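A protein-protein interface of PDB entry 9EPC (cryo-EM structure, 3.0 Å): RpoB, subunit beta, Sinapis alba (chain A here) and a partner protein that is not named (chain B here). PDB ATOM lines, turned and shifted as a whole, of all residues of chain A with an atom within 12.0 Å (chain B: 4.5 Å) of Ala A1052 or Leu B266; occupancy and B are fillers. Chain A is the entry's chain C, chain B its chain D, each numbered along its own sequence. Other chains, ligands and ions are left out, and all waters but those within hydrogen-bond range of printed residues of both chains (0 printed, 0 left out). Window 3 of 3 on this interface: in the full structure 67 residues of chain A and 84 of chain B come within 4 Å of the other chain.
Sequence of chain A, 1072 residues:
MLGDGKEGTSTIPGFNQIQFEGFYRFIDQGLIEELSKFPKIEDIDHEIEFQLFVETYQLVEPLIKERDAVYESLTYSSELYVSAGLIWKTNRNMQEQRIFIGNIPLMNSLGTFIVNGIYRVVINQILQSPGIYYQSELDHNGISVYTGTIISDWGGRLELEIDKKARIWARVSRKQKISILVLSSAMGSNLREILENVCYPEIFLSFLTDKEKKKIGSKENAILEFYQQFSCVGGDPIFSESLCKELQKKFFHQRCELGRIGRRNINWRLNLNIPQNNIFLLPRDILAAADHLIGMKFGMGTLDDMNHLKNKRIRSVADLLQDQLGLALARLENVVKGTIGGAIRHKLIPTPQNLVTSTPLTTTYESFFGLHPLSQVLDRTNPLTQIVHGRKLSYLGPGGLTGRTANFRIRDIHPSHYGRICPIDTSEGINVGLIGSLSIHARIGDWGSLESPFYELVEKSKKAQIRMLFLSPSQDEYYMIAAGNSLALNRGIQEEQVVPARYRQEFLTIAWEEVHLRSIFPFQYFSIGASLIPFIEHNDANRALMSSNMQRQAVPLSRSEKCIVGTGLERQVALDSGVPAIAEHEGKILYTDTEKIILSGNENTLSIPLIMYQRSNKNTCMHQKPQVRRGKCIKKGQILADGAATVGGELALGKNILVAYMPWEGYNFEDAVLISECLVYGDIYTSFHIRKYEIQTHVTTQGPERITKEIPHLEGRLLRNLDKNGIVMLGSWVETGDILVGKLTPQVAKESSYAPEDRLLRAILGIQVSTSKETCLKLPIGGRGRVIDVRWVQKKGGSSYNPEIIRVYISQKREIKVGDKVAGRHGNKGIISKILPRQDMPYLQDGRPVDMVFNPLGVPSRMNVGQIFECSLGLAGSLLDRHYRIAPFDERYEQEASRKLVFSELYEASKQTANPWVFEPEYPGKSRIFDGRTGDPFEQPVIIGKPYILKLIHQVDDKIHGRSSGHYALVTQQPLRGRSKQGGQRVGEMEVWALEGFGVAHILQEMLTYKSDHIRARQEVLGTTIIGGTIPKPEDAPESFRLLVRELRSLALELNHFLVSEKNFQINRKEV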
ATOM      1  N   LEU A1043     -14.727  -1.719  -0.456  1.00  0.00           N
ATOM      2  CA  LEU A1043     -13.307  -1.398  -0.544  1.00  0.00           C
ATOM      3  C   LEU A1043     -12.618  -2.248  -1.603  1.00  0.00           C
ATOM      4  O   LEU A1043     -11.721  -1.770  -2.306  1.00  0.00           O
ATOM      5  CB  LEU A1043     -12.637  -1.588   0.816  1.00  0.00           C
ATOM      6  CG  LEU A1043     -12.441  -0.331   1.667  1.00  0.00           C
ATOM      7  CD1 LEU A1043     -13.764   0.366   1.937  1.00  0.00           C
ATOM      8  CD2 LEU A1043     -11.737  -0.676   2.970  1.00  0.00           C
ATOM      9  N   LEU A1044     -13.022  -3.514  -1.728  1.00  0.00           N
ATOM     10  CA  LEU A1044     -12.431  -4.378  -2.745  1.00  0.00           C
ATOM     11  C   LEU A1044     -12.719  -3.858  -4.145  1.00  0.00           C
ATOM     12  O   LEU A1044     -11.854  -3.916  -5.027  1.00  0.00           O
ATOM     13  CB  LEU A1044     -12.951  -5.806  -2.590  1.00  0.00           C
ATOM     14  CG  LEU A1044     -12.462  -6.795  -3.648  1.00  0.00           C
ATOM     15  CD1 LEU A1044     -10.947  -6.897  -3.620  1.00  0.00           C
ATOM     16  CD2 LEU A1044     -13.096  -8.159  -3.448  1.00  0.00           C
ATOM     17  N   VAL A1045     -13.931  -3.349  -4.370  1.00  0.00           N
ATOM     18  CA  VAL A1045     -14.283  -2.825  -5.686  1.00  0.00           C
ATOM     19  C   VAL A1045     -13.380  -1.657  -6.056  1.00  0.00           C
ATOM     20  O   VAL A1045     -12.879  -1.576  -7.183  1.00  0.00           O
ATOM     21  CB  VAL A1045     -15.769  -2.425  -5.721  1.00  0.00           C
ATOM     22  CG1 VAL A1045     -16.085  -1.675  -7.003  1.00  0.00           C
ATOM     23  CG2 VAL A1045     -16.642  -3.657  -5.600  1.00  0.00           C
ATOM     24  N   ARG A1046     -13.144  -0.745  -5.109  1.00  0.00           N
ATOM     25  CA  ARG A1046     -12.314   0.420  -5.397  1.00  0.00           C
ATOM     26  C   ARG A1046     -10.900   0.009  -5.783  1.00  0.00           C
ATOM     27  O   ARG A1046     -10.305   0.588  -6.699  1.00  0.00           O
ATOM     28  CB  ARG A1046     -12.283   1.356  -4.191  1.00  0.00           C
ATOM     29  CG  ARG A1046     -13.638   1.607  -3.563  1.00  0.00           C
ATOM     30  CD  ARG A1046     -14.617   2.211  -4.549  1.00  0.00           C
ATOM     31  NE  ARG A1046     -15.964   2.265  -3.995  1.00  0.00           N
ATOM     32  CZ  ARG A1046     -17.003   2.813  -4.606  1.00  0.00           C
ATOM     33  NH1 ARG A1046     -16.886   3.376  -5.796  1.00  0.00           N
ATOM     34  NH2 ARG A1046     -18.190   2.798  -4.006  1.00  0.00           N
ATOM     35  N   GLU A1047     -10.344  -0.987  -5.091  1.00  0.00           N
ATOM     36  CA  GLU A1047      -9.010  -1.464  -5.435  1.00  0.00           C
ATOM     37  C   GLU A1047      -8.980  -2.038  -6.846  1.00  0.00           C
ATOM     38  O   GLU A1047      -8.047  -1.772  -7.612  1.00  0.00           O
ATOM     39  CB  GLU A1047      -8.549  -2.504  -4.418  1.00  0.00           C
ATOM     40  CG  GLU A1047      -8.345  -1.942  -3.024  1.00  0.00           C
ATOM     41  CD  GLU A1047      -8.161  -3.025  -1.984  1.00  0.00           C
ATOM     42  OE1 GLU A1047      -8.779  -4.100  -2.134  1.00  0.00           O
ATOM     43  OE2 GLU A1047      -7.397  -2.805  -1.022  1.00  0.00           O
ATOM     44  N   LEU A1048      -9.994  -2.825  -7.208  1.00  0.00           N
ATOM     45  CA  LEU A1048     -10.096  -3.286  -8.587  1.00  0.00           C
ATOM     46  C   LEU A1048     -10.473  -2.147  -9.522  1.00  0.00           C
ATOM     47  O   LEU A1048     -10.042  -2.128 -10.681  1.00  0.00           O
ATOM     48  CB  LEU A1048     -11.112  -4.420  -8.692  1.00  0.00           C
ATOM     49  CG  LEU A1048     -10.787  -5.652  -7.853  1.00  0.00           C
ATOM     50  CD1 LEU A1048     -11.752  -6.780  -8.165  1.00  0.00           C
ATOM     51  CD2 LEU A1048      -9.352  -6.083  -8.086  1.00  0.00           C
ATOM     52  N   ARG A1049     -11.275  -1.196  -9.042  1.00  0.00           N
ATOM     53  CA  ARG A1049     -11.592  -0.023  -9.845  1.00  0.00           C
ATOM     54  C   ARG A1049     -10.346   0.801 -10.131  1.00  0.00           C
ATOM     55  O   ARG A1049     -10.262   1.460 -11.174  1.00  0.00           O
ATOM     56  CB  ARG A1049     -12.653   0.820  -9.137  1.00  0.00           C
ATOM     57  CG  ARG A1049     -13.208   1.954  -9.962  1.00  0.00           C
ATOM     58  CD  ARG A1049     -14.515   2.473  -9.392  1.00  0.00           C
ATOM     59  NE  ARG A1049     -15.554   1.452  -9.392  1.00  0.00           N
ATOM     60  CZ  ARG A1049     -16.822   1.675  -9.079  1.00  0.00           C
ATOM     61  NH1 ARG A1049     -17.248   2.881  -8.743  1.00  0.00           N
ATOM     62  NH2 ARG A1049     -17.685   0.664  -9.107  1.00  0.00           N
ATOM     63  N   SER A1050      -9.367   0.770  -9.227  1.00  0.00           N
ATOM     64  CA  SER A1050      -8.108   1.464  -9.462  1.00  0.00           C
ATOM     65  C   SER A1050      -7.235   0.744 -10.480  1.00  0.00           C
ATOM     66  O   SER A1050      -6.347   1.369 -11.068  1.00  0.00           O
ATOM     67  CB  SER A1050      -7.346   1.624  -8.149  1.00  0.00           C
ATOM     68  OG  SER A1050      -7.110   0.363  -7.550  1.00  0.00           O
ATOM     69  N   LEU A1051      -7.462  -0.551 -10.697  1.00  0.00           N
ATOM     70  CA  LEU A1051      -6.728  -1.324 -11.692  1.00  0.00           C
ATOM     71  C   LEU A1051      -7.449  -1.387 -13.029  1.00  0.00           C
ATOM     72  O   LEU A1051      -7.271  -2.355 -13.780  1.00  0.00           O
ATOM     73  CB  LEU A1051      -6.461  -2.736 -11.169  1.00  0.00           C
ATOM     74  CG  LEU A1051      -5.330  -2.887 -10.156  1.00  0.00           C
ATOM     75  CD1 LEU A1051      -5.328  -4.287  -9.575  1.00  0.00           C
ATOM     76  CD2 LEU A1051      -4.000  -2.580 -10.816  1.00  0.00           C
ATOM     77  N   ALA A1052      -8.271  -0.382 -13.337  1.00  0.00           N
ATOM     78  CA  ALA A1052      -9.030  -0.323 -14.584  1.00  0.00           C
ATOM     79  C   ALA A1052      -9.944  -1.533 -14.752  1.00  0.00           C
ATOM     80  O   ALA A1052     -10.185  -1.990 -15.871  1.00  0.00           O
ATOM     81  CB  ALA A1052      -8.106  -0.177 -15.796  1.00  0.00           C
ATOM     82  N   LEU A1053     -10.460  -2.059 -13.646  1.00  0.00           N
ATOM     83  CA  LEU A1053     -11.387  -3.181 -13.662  1.00  0.00           C
ATOM     84  C   LEU A1053     -12.702  -2.744 -13.038  1.00  0.00           C
ATOM     85  O   LEU A1053     -12.719  -2.228 -11.917  1.00  0.00           O
ATOM     86  CB  LEU A1053     -10.816  -4.380 -12.903  1.00  0.00           C
ATOM     87  CG  LEU A1053      -9.436  -4.859 -13.345  1.00  0.00           C
ATOM     88  CD1 LEU A1053      -9.044  -6.118 -12.592  1.00  0.00           C
ATOM     89  CD2 LEU A1053      -9.409  -5.094 -14.841  1.00  0.00           C
ATOM     90  N   GLU A1054     -13.796  -2.953 -13.762  1.00  0.00           N
ATOM     91  CA  GLU A1054     -15.122  -2.555 -13.311  1.00  0.00           C
ATOM     92  C   GLU A1054     -15.848  -3.785 -12.785  1.00  0.00           C
ATOM     93  O   GLU A1054     -16.249  -4.656 -13.563  1.00  0.00           O
ATOM     94  CB  GLU A1054     -15.906  -1.899 -14.445  1.00  0.00           C
ATOM     95  CG  GLU A1054     -17.312  -1.486 -14.061  1.00  0.00           C
ATOM     96  CD  GLU A1054     -18.069  -0.852 -15.211  1.00  0.00           C
ATOM     97  OE1 GLU A1054     -17.439  -0.563 -16.249  1.00  0.00           O
ATOM     98  OE2 GLU A1054     -19.293  -0.646 -15.077  1.00  0.00           O
ATOM     99  N   LEU A1055     -16.019  -3.854 -11.469  1.00  0.00           N
ATOM    100  CA  LEU A1055     -16.720  -4.957 -10.821  1.00  0.00           C
ATOM    101  C   LEU A1055     -18.154  -4.521 -10.554  1.00  0.00           C
ATOM    102  O   LEU A1055     -18.398  -3.645  -9.717  1.00  0.00           O
ATOM    103  CB  LEU A1055     -16.016  -5.364  -9.531  1.00  0.00           C
ATOM    104  CG  LEU A1055     -16.549  -6.621  -8.847  1.00  0.00           C
ATOM    105  CD1 LEU A1055     -16.415  -7.820  -9.766  1.00  0.00           C
ATOM    106  CD2 LEU A1055     -15.820  -6.863  -7.539  1.00  0.00           C
ATOM    107  N   ASN A1056     -19.100  -5.129 -11.261  1.00  0.00           N
ATOM    108  CA  ASN A1056     -20.506  -4.770 -11.171  1.00  0.00           C
ATOM    109  C   ASN A1056     -21.306  -5.924 -10.591  1.00  0.00           C
ATOM    110  O   ASN A1056     -21.110  -7.082 -10.971  1.00  0.00           O
ATOM    111  CB  ASN A1056     -21.062  -4.399 -12.545  1.00  0.00           C
ATOM    112  CG  ASN A1056     -20.360  -3.208 -13.153  1.00  0.00           C
ATOM    113  OD1 ASN A1056     -20.003  -2.261 -12.451  1.00  0.00           O
ATOM    114  ND2 ASN A1056     -20.157  -3.246 -14.464  1.00  0.00           N
ATOM    115  N   GLY B  13     -14.702  -6.563 -15.827  1.00  0.00           N
ATOM    116  CA  GLY B  13     -14.157  -6.299 -17.145  1.00  0.00           C
ATOM    117  C   GLY B  13     -13.388  -5.000 -17.159  1.00  0.00           C
ATOM    118  O   GLY B  13     -13.428  -4.213 -16.206  1.00  0.00           O
ATOM    119  N   LEU B  14     -12.677  -4.787 -18.263  1.00  0.00           N
ATOM    120  CA  LEU B  14     -11.985  -3.527 -18.471  1.00  0.00           C
ATOM    121  C   LEU B  14     -12.988  -2.392 -18.618  1.00  0.00           C
ATOM    122  O   LEU B  14     -14.119  -2.585 -19.073  1.00  0.00           O
ATOM    123  CB  LEU B  14     -11.092  -3.597 -19.708  1.00  0.00           C
ATOM    124  CG  LEU B  14      -9.776  -4.351 -19.542  1.00  0.00           C
ATOM    125  CD1 LEU B  14      -8.927  -4.207 -20.788  1.00  0.00           C
ATOM    126  CD2 LEU B  14      -9.027  -3.841 -18.326  1.00  0.00           C
ATOM    127  N   VAL B  15     -12.562  -1.196 -18.228  1.00  0.00           N
ATOM    128  CA  VAL B  15     -13.429  -0.029 -18.167  1.00  0.00           C
ATOM    129  C   VAL B  15     -13.010   0.952 -19.252  1.00  0.00           C
ATOM    130  O   VAL B  15     -11.816   1.216 -19.435  1.00  0.00           O
ATOM    131  CB  VAL B  15     -13.384   0.623 -16.776  1.00  0.00           C
ATOM    132  CG1 VAL B  15     -11.950   0.826 -16.330  1.00  0.00           C
ATOM    133  CG2 VAL B  15     -14.120   1.939 -16.788  1.00  0.00           C
ATOM    134  N   PRO B 112      -0.944   7.865 -24.148  1.00  0.00           N
ATOM    135  CA  PRO B 112      -1.525   6.608 -23.671  1.00  0.00           C
ATOM    136  C   PRO B 112      -0.469   5.711 -23.050  1.00  0.00           C
ATOM    137  O   PRO B 112       0.715   5.777 -23.386  1.00  0.00           O
ATOM    138  CB  PRO B 112      -2.111   5.984 -24.941  1.00  0.00           C
ATOM    139  CG  PRO B 112      -1.324   6.589 -26.047  1.00  0.00           C
ATOM    140  CD  PRO B 112      -1.008   7.984 -25.612  1.00  0.00           C
ATOM    141  N   VAL B 113      -0.914   4.875 -22.116  1.00  0.00           N
ATOM    142  CA  VAL B 113      -0.043   3.960 -21.391  1.00  0.00           C
ATOM    143  C   VAL B 113      -0.636   2.562 -21.464  1.00  0.00           C
ATOM    144  O   VAL B 113      -1.825   2.373 -21.187  1.00  0.00           O
ATOM    145  CB  VAL B 113       0.140   4.394 -19.925  1.00  0.00           C
ATOM    146  CG1 VAL B 113       0.627   3.231 -19.086  1.00  0.00           C
ATOM    147  CG2 VAL B 113       1.114   5.553 -19.844  1.00  0.00           C
ATOM    148  N   HIS B 115      -1.521  -1.102 -20.278  1.00  0.00           N
ATOM    149  CA  HIS B 115      -1.763  -1.772 -19.008  1.00  0.00           C
ATOM    150  C   HIS B 115      -0.834  -2.973 -18.910  1.00  0.00           C
ATOM    151  O   HIS B 115      -0.910  -3.894 -19.731  1.00  0.00           O
ATOM    152  CB  HIS B 115      -3.225  -2.195 -18.900  1.00  0.00           C
ATOM    153  CG  HIS B 115      -3.646  -2.572 -17.515  1.00  0.00           C
ATOM    154  ND1 HIS B 115      -2.760  -3.024 -16.562  1.00  0.00           N
ATOM    155  CD2 HIS B 115      -4.862  -2.560 -16.921  1.00  0.00           C
ATOM    156  CE1 HIS B 115      -3.411  -3.278 -15.442  1.00  0.00           C
ATOM    157  NE2 HIS B 115      -4.689  -3.002 -15.632  1.00  0.00           N
ATOM    158  N   TRP B 263      -9.088  -0.619 -24.682  1.00  0.00           N
ATOM    159  CA  TRP B 263      -9.067  -0.348 -23.253  1.00  0.00           C
ATOM    160  C   TRP B 263      -7.864  -0.978 -22.565  1.00  0.00           C
ATOM    161  O   TRP B 263      -7.546  -0.597 -21.434  1.00  0.00           O
ATOM    162  CB  TRP B 263     -10.367  -0.836 -22.616  1.00  0.00           C
ATOM    163  CG  TRP B 263     -11.599  -0.248 -23.247  1.00  0.00           C
ATOM    164  CD1 TRP B 263     -11.650   0.760 -24.164  1.00  0.00           C
ATOM    165  CD2 TRP B 263     -12.953  -0.638 -23.007  1.00  0.00           C
ATOM    166  NE1 TRP B 263     -12.950   1.021 -24.510  1.00  0.00           N
ATOM    167  CE2 TRP B 263     -13.771   0.176 -23.811  1.00  0.00           C
ATOM    168  CE3 TRP B 263     -13.555  -1.595 -22.189  1.00  0.00           C
ATOM    169  CZ2 TRP B 263     -15.155   0.059 -23.824  1.00  0.00           C
ATOM    170  CZ3 TRP B 263     -14.928  -1.707 -22.201  1.00  0.00           C
ATOM    171  CH2 TRP B 263     -15.714  -0.884 -23.012  1.00  0.00           C
ATOM    172  N   MET B 264      -7.189  -1.925 -23.219  1.00  0.00           N
ATOM    173  CA  MET B 264      -5.937  -2.443 -22.684  1.00  0.00           C
ATOM    174  C   MET B 264      -4.853  -1.377 -22.642  1.00  0.00           C
ATOM    175  O   MET B 264      -3.882  -1.524 -21.895  1.00  0.00           O
ATOM    176  CB  MET B 264      -5.458  -3.640 -23.506  1.00  0.00           C
ATOM    177  CG  MET B 264      -6.247  -4.913 -23.267  1.00  0.00           C
ATOM    178  SD  MET B 264      -5.603  -6.326 -24.181  1.00  0.00           S
ATOM    179  CE  MET B 264      -5.942  -5.822 -25.862  1.00  0.00           C
ATOM    180  N   VAL B 265      -4.992  -0.319 -23.429  1.00  0.00           N
ATOM    181  CA  VAL B 265      -4.080   0.816 -23.402  1.00  0.00           C
ATOM    182  C   VAL B 265      -4.889   2.006 -22.909  1.00  0.00           C
ATOM    183  O   VAL B 265      -5.630   2.630 -23.677  1.00  0.00           O
ATOM    184  CB  VAL B 265      -3.458   1.084 -24.775  1.00  0.00           C
ATOM    185  CG1 VAL B 265      -2.451   2.217 -24.684  1.00  0.00           C
ATOM    186  CG2 VAL B 265      -2.808  -0.177 -25.310  1.00  0.00           C
ATOM    187  N   LEU B 266      -4.754   2.325 -21.628  1.00  0.00           N
ATOM    188  CA  LEU B 266      -5.576   3.350 -21.005  1.00  0.00           C
ATOM    189  C   LEU B 266      -4.985   4.734 -21.227  1.00  0.00           C
ATOM    190  O   LEU B 266      -3.767   4.919 -21.196  1.00  0.00           O
ATOM    191  CB  LEU B 266      -5.735   3.076 -19.508  1.00  0.00           C
ATOM    192  CG  LEU B 266      -4.590   2.383 -18.766  1.00  0.00           C
ATOM    193  CD1 LEU B 266      -3.444   3.335 -18.485  1.00  0.00           C
ATOM    194  CD2 LEU B 266      -5.100   1.770 -17.475  1.00  0.00           C
ATOM    195  N   CYS B 267      -5.865   5.704 -21.472  1.00  0.00           N
ATOM    196  CA  CYS B 267      -5.482   7.105 -21.541  1.00  0.00           C
ATOM    197  C   CYS B 267      -5.871   7.881 -20.292  1.00  0.00           C
ATOM    198  O   CYS B 267      -5.437   9.026 -20.131  1.00  0.00           O
ATOM    199  CB  CYS B 267      -6.107   7.766 -22.775  1.00  0.00           C
ATOM    200  SG  CYS B 267      -7.889   7.532 -22.925  1.00  0.00           S
ATOM    201  N   LEU B 268      -6.676   7.289 -19.414  1.00  0.00           N
ATOM    202  CA  LEU B 268      -7.016   7.865 -18.123  1.00  0.00           C
ATOM    203  C   LEU B 268      -6.669   6.870 -17.026  1.00  0.00           C
ATOM    204  O   LEU B 268      -6.894   5.665 -17.166  1.00  0.00           O
ATOM    205  CB  LEU B 268      -8.500   8.228 -18.040  1.00  0.00           C
ATOM    206  CG  LEU B 268      -9.011   9.265 -19.038  1.00  0.00           C
ATOM    207  CD1 LEU B 268     -10.470   9.581 -18.765  1.00  0.00           C
ATOM    208  CD2 LEU B 268      -8.165  10.523 -18.980  1.00  0.00           C
ATOM    209  N   PRO B 270      -7.354   5.827 -13.165  1.00  0.00           N
ATOM    210  CA  PRO B 270      -8.145   6.022 -11.947  1.00  0.00           C
ATOM    211  C   PRO B 270      -7.259   6.144 -10.720  1.00  0.00           C
ATOM    212  O   PRO B 270      -6.155   5.596 -10.662  1.00  0.00           O
ATOM    213  CB  PRO B 270      -9.014   4.762 -11.884  1.00  0.00           C
ATOM    214  CG  PRO B 270      -8.254   3.748 -12.659  1.00  0.00           C
ATOM    215  CD  PRO B 270      -7.577   4.501 -13.762  1.00  0.00           C
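A ring nitrogen (NE2) of His B115 sits at hydrogen-bond distance from the backbone carbonyl oxygen of Leu A1051, at 3.2 Å. The backbone carbonyl oxygen (O) of Ala A1052 sits close to the backbone NH (N) of Val B15, 3.4 Å away. O of Gly B13 is in hydrogen-bond range of N of Glu A1054.
Of the printed residues of chain B, Arg A1049 touches Pro B270. Printed residues of chain B within 4 Å of Ser A1050: Pro B270 (3.4 Å). Of the printed residues of chain B, Leu A1051 touches His B115. Ala A1052 touches just these residues of chain B: Gly B13 (3.9 Å), Leu B14 (3.3 Å), Val B15 (3.4 Å) and Leu B266 (3.96 Å). Printed residues of chain B within 4 Å of Glu A1054: Gly B13. Asn A1056 touches none of the printed residues of chain B. Of chain A, only Ala A1052, Leu A1053 and Glu A1054 come within 4 Å of Gly B13. Of chain A, only Ala A1052 (3.3 Å) and Leu A1053 (3.7 Å) come within 4 Å of Leu B14. No residue of chain A comes within 4 Å of Pro B112. His B115 touches one residue of chain A. Met B264 touches none of the printed residues of chain A. Leu B266 touches just one residue of chain A: Ala A1052 (3.96 Å). No residue of chain A comes within 4 Å of Cys B267. No residue of chain A comes within 4 Å of Leu B268. The nearest printed residue of chain B that does not touch Ala A1052 is His B115 (4.2 Å). The nearest residue of chain A that does not touch Leu B266 is Leu A1051 (5.9 Å).
O of Arg A1046 is in hydrogen-bond range of OG of Ser A1050, at 3.3 Å. The backbone carbonyl oxygen (O) of Leu A1048 is in hydrogen-bond range of the backbone NH (N) of Leu A1053 (3.0 Å). ND2 of Asn A1056 lies within hydrogen-bond range of OE2 of Glu A1054 (2.8 Å). O of Val B113 sits at hydrogen-bond distance from N of Leu B266. The backbone NH (N) of His B115 is in hydrogen-bond range of the backbone carbonyl oxygen (O) of Met B264, 2.9 Å away.
O of Arg A1049 touches CG of Pro B270 (3.4 Å). Ser A1050 touches Pro B270 (O to CG, 3.4 Å). Gly B13 touches Ala A1052. Ala A1052 touches Leu B14. CB of Ala A1052 touches CD2 of Leu B266, at 3.96 Å. CA of Leu A1053 touches O of Gly B13, 3.4 Å away. Leu A1053 touches Leu B14 (CD2 to CD2, 3.7 Å).
Printed residues of chain A that touch a printed residue of chain B: Arg A1049, Ser A1050, Leu A1051, Ala A1052, Leu A1053 and Glu A1054. Of the 13 printed residues of chain B, 6 touch a printed residue of chain A. Hydrophobic or aromatic side chains of chain B within 4 Å of the printed part of chain A: Leu B14, Val B15, His B115, Leu B266 and Pro B270.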
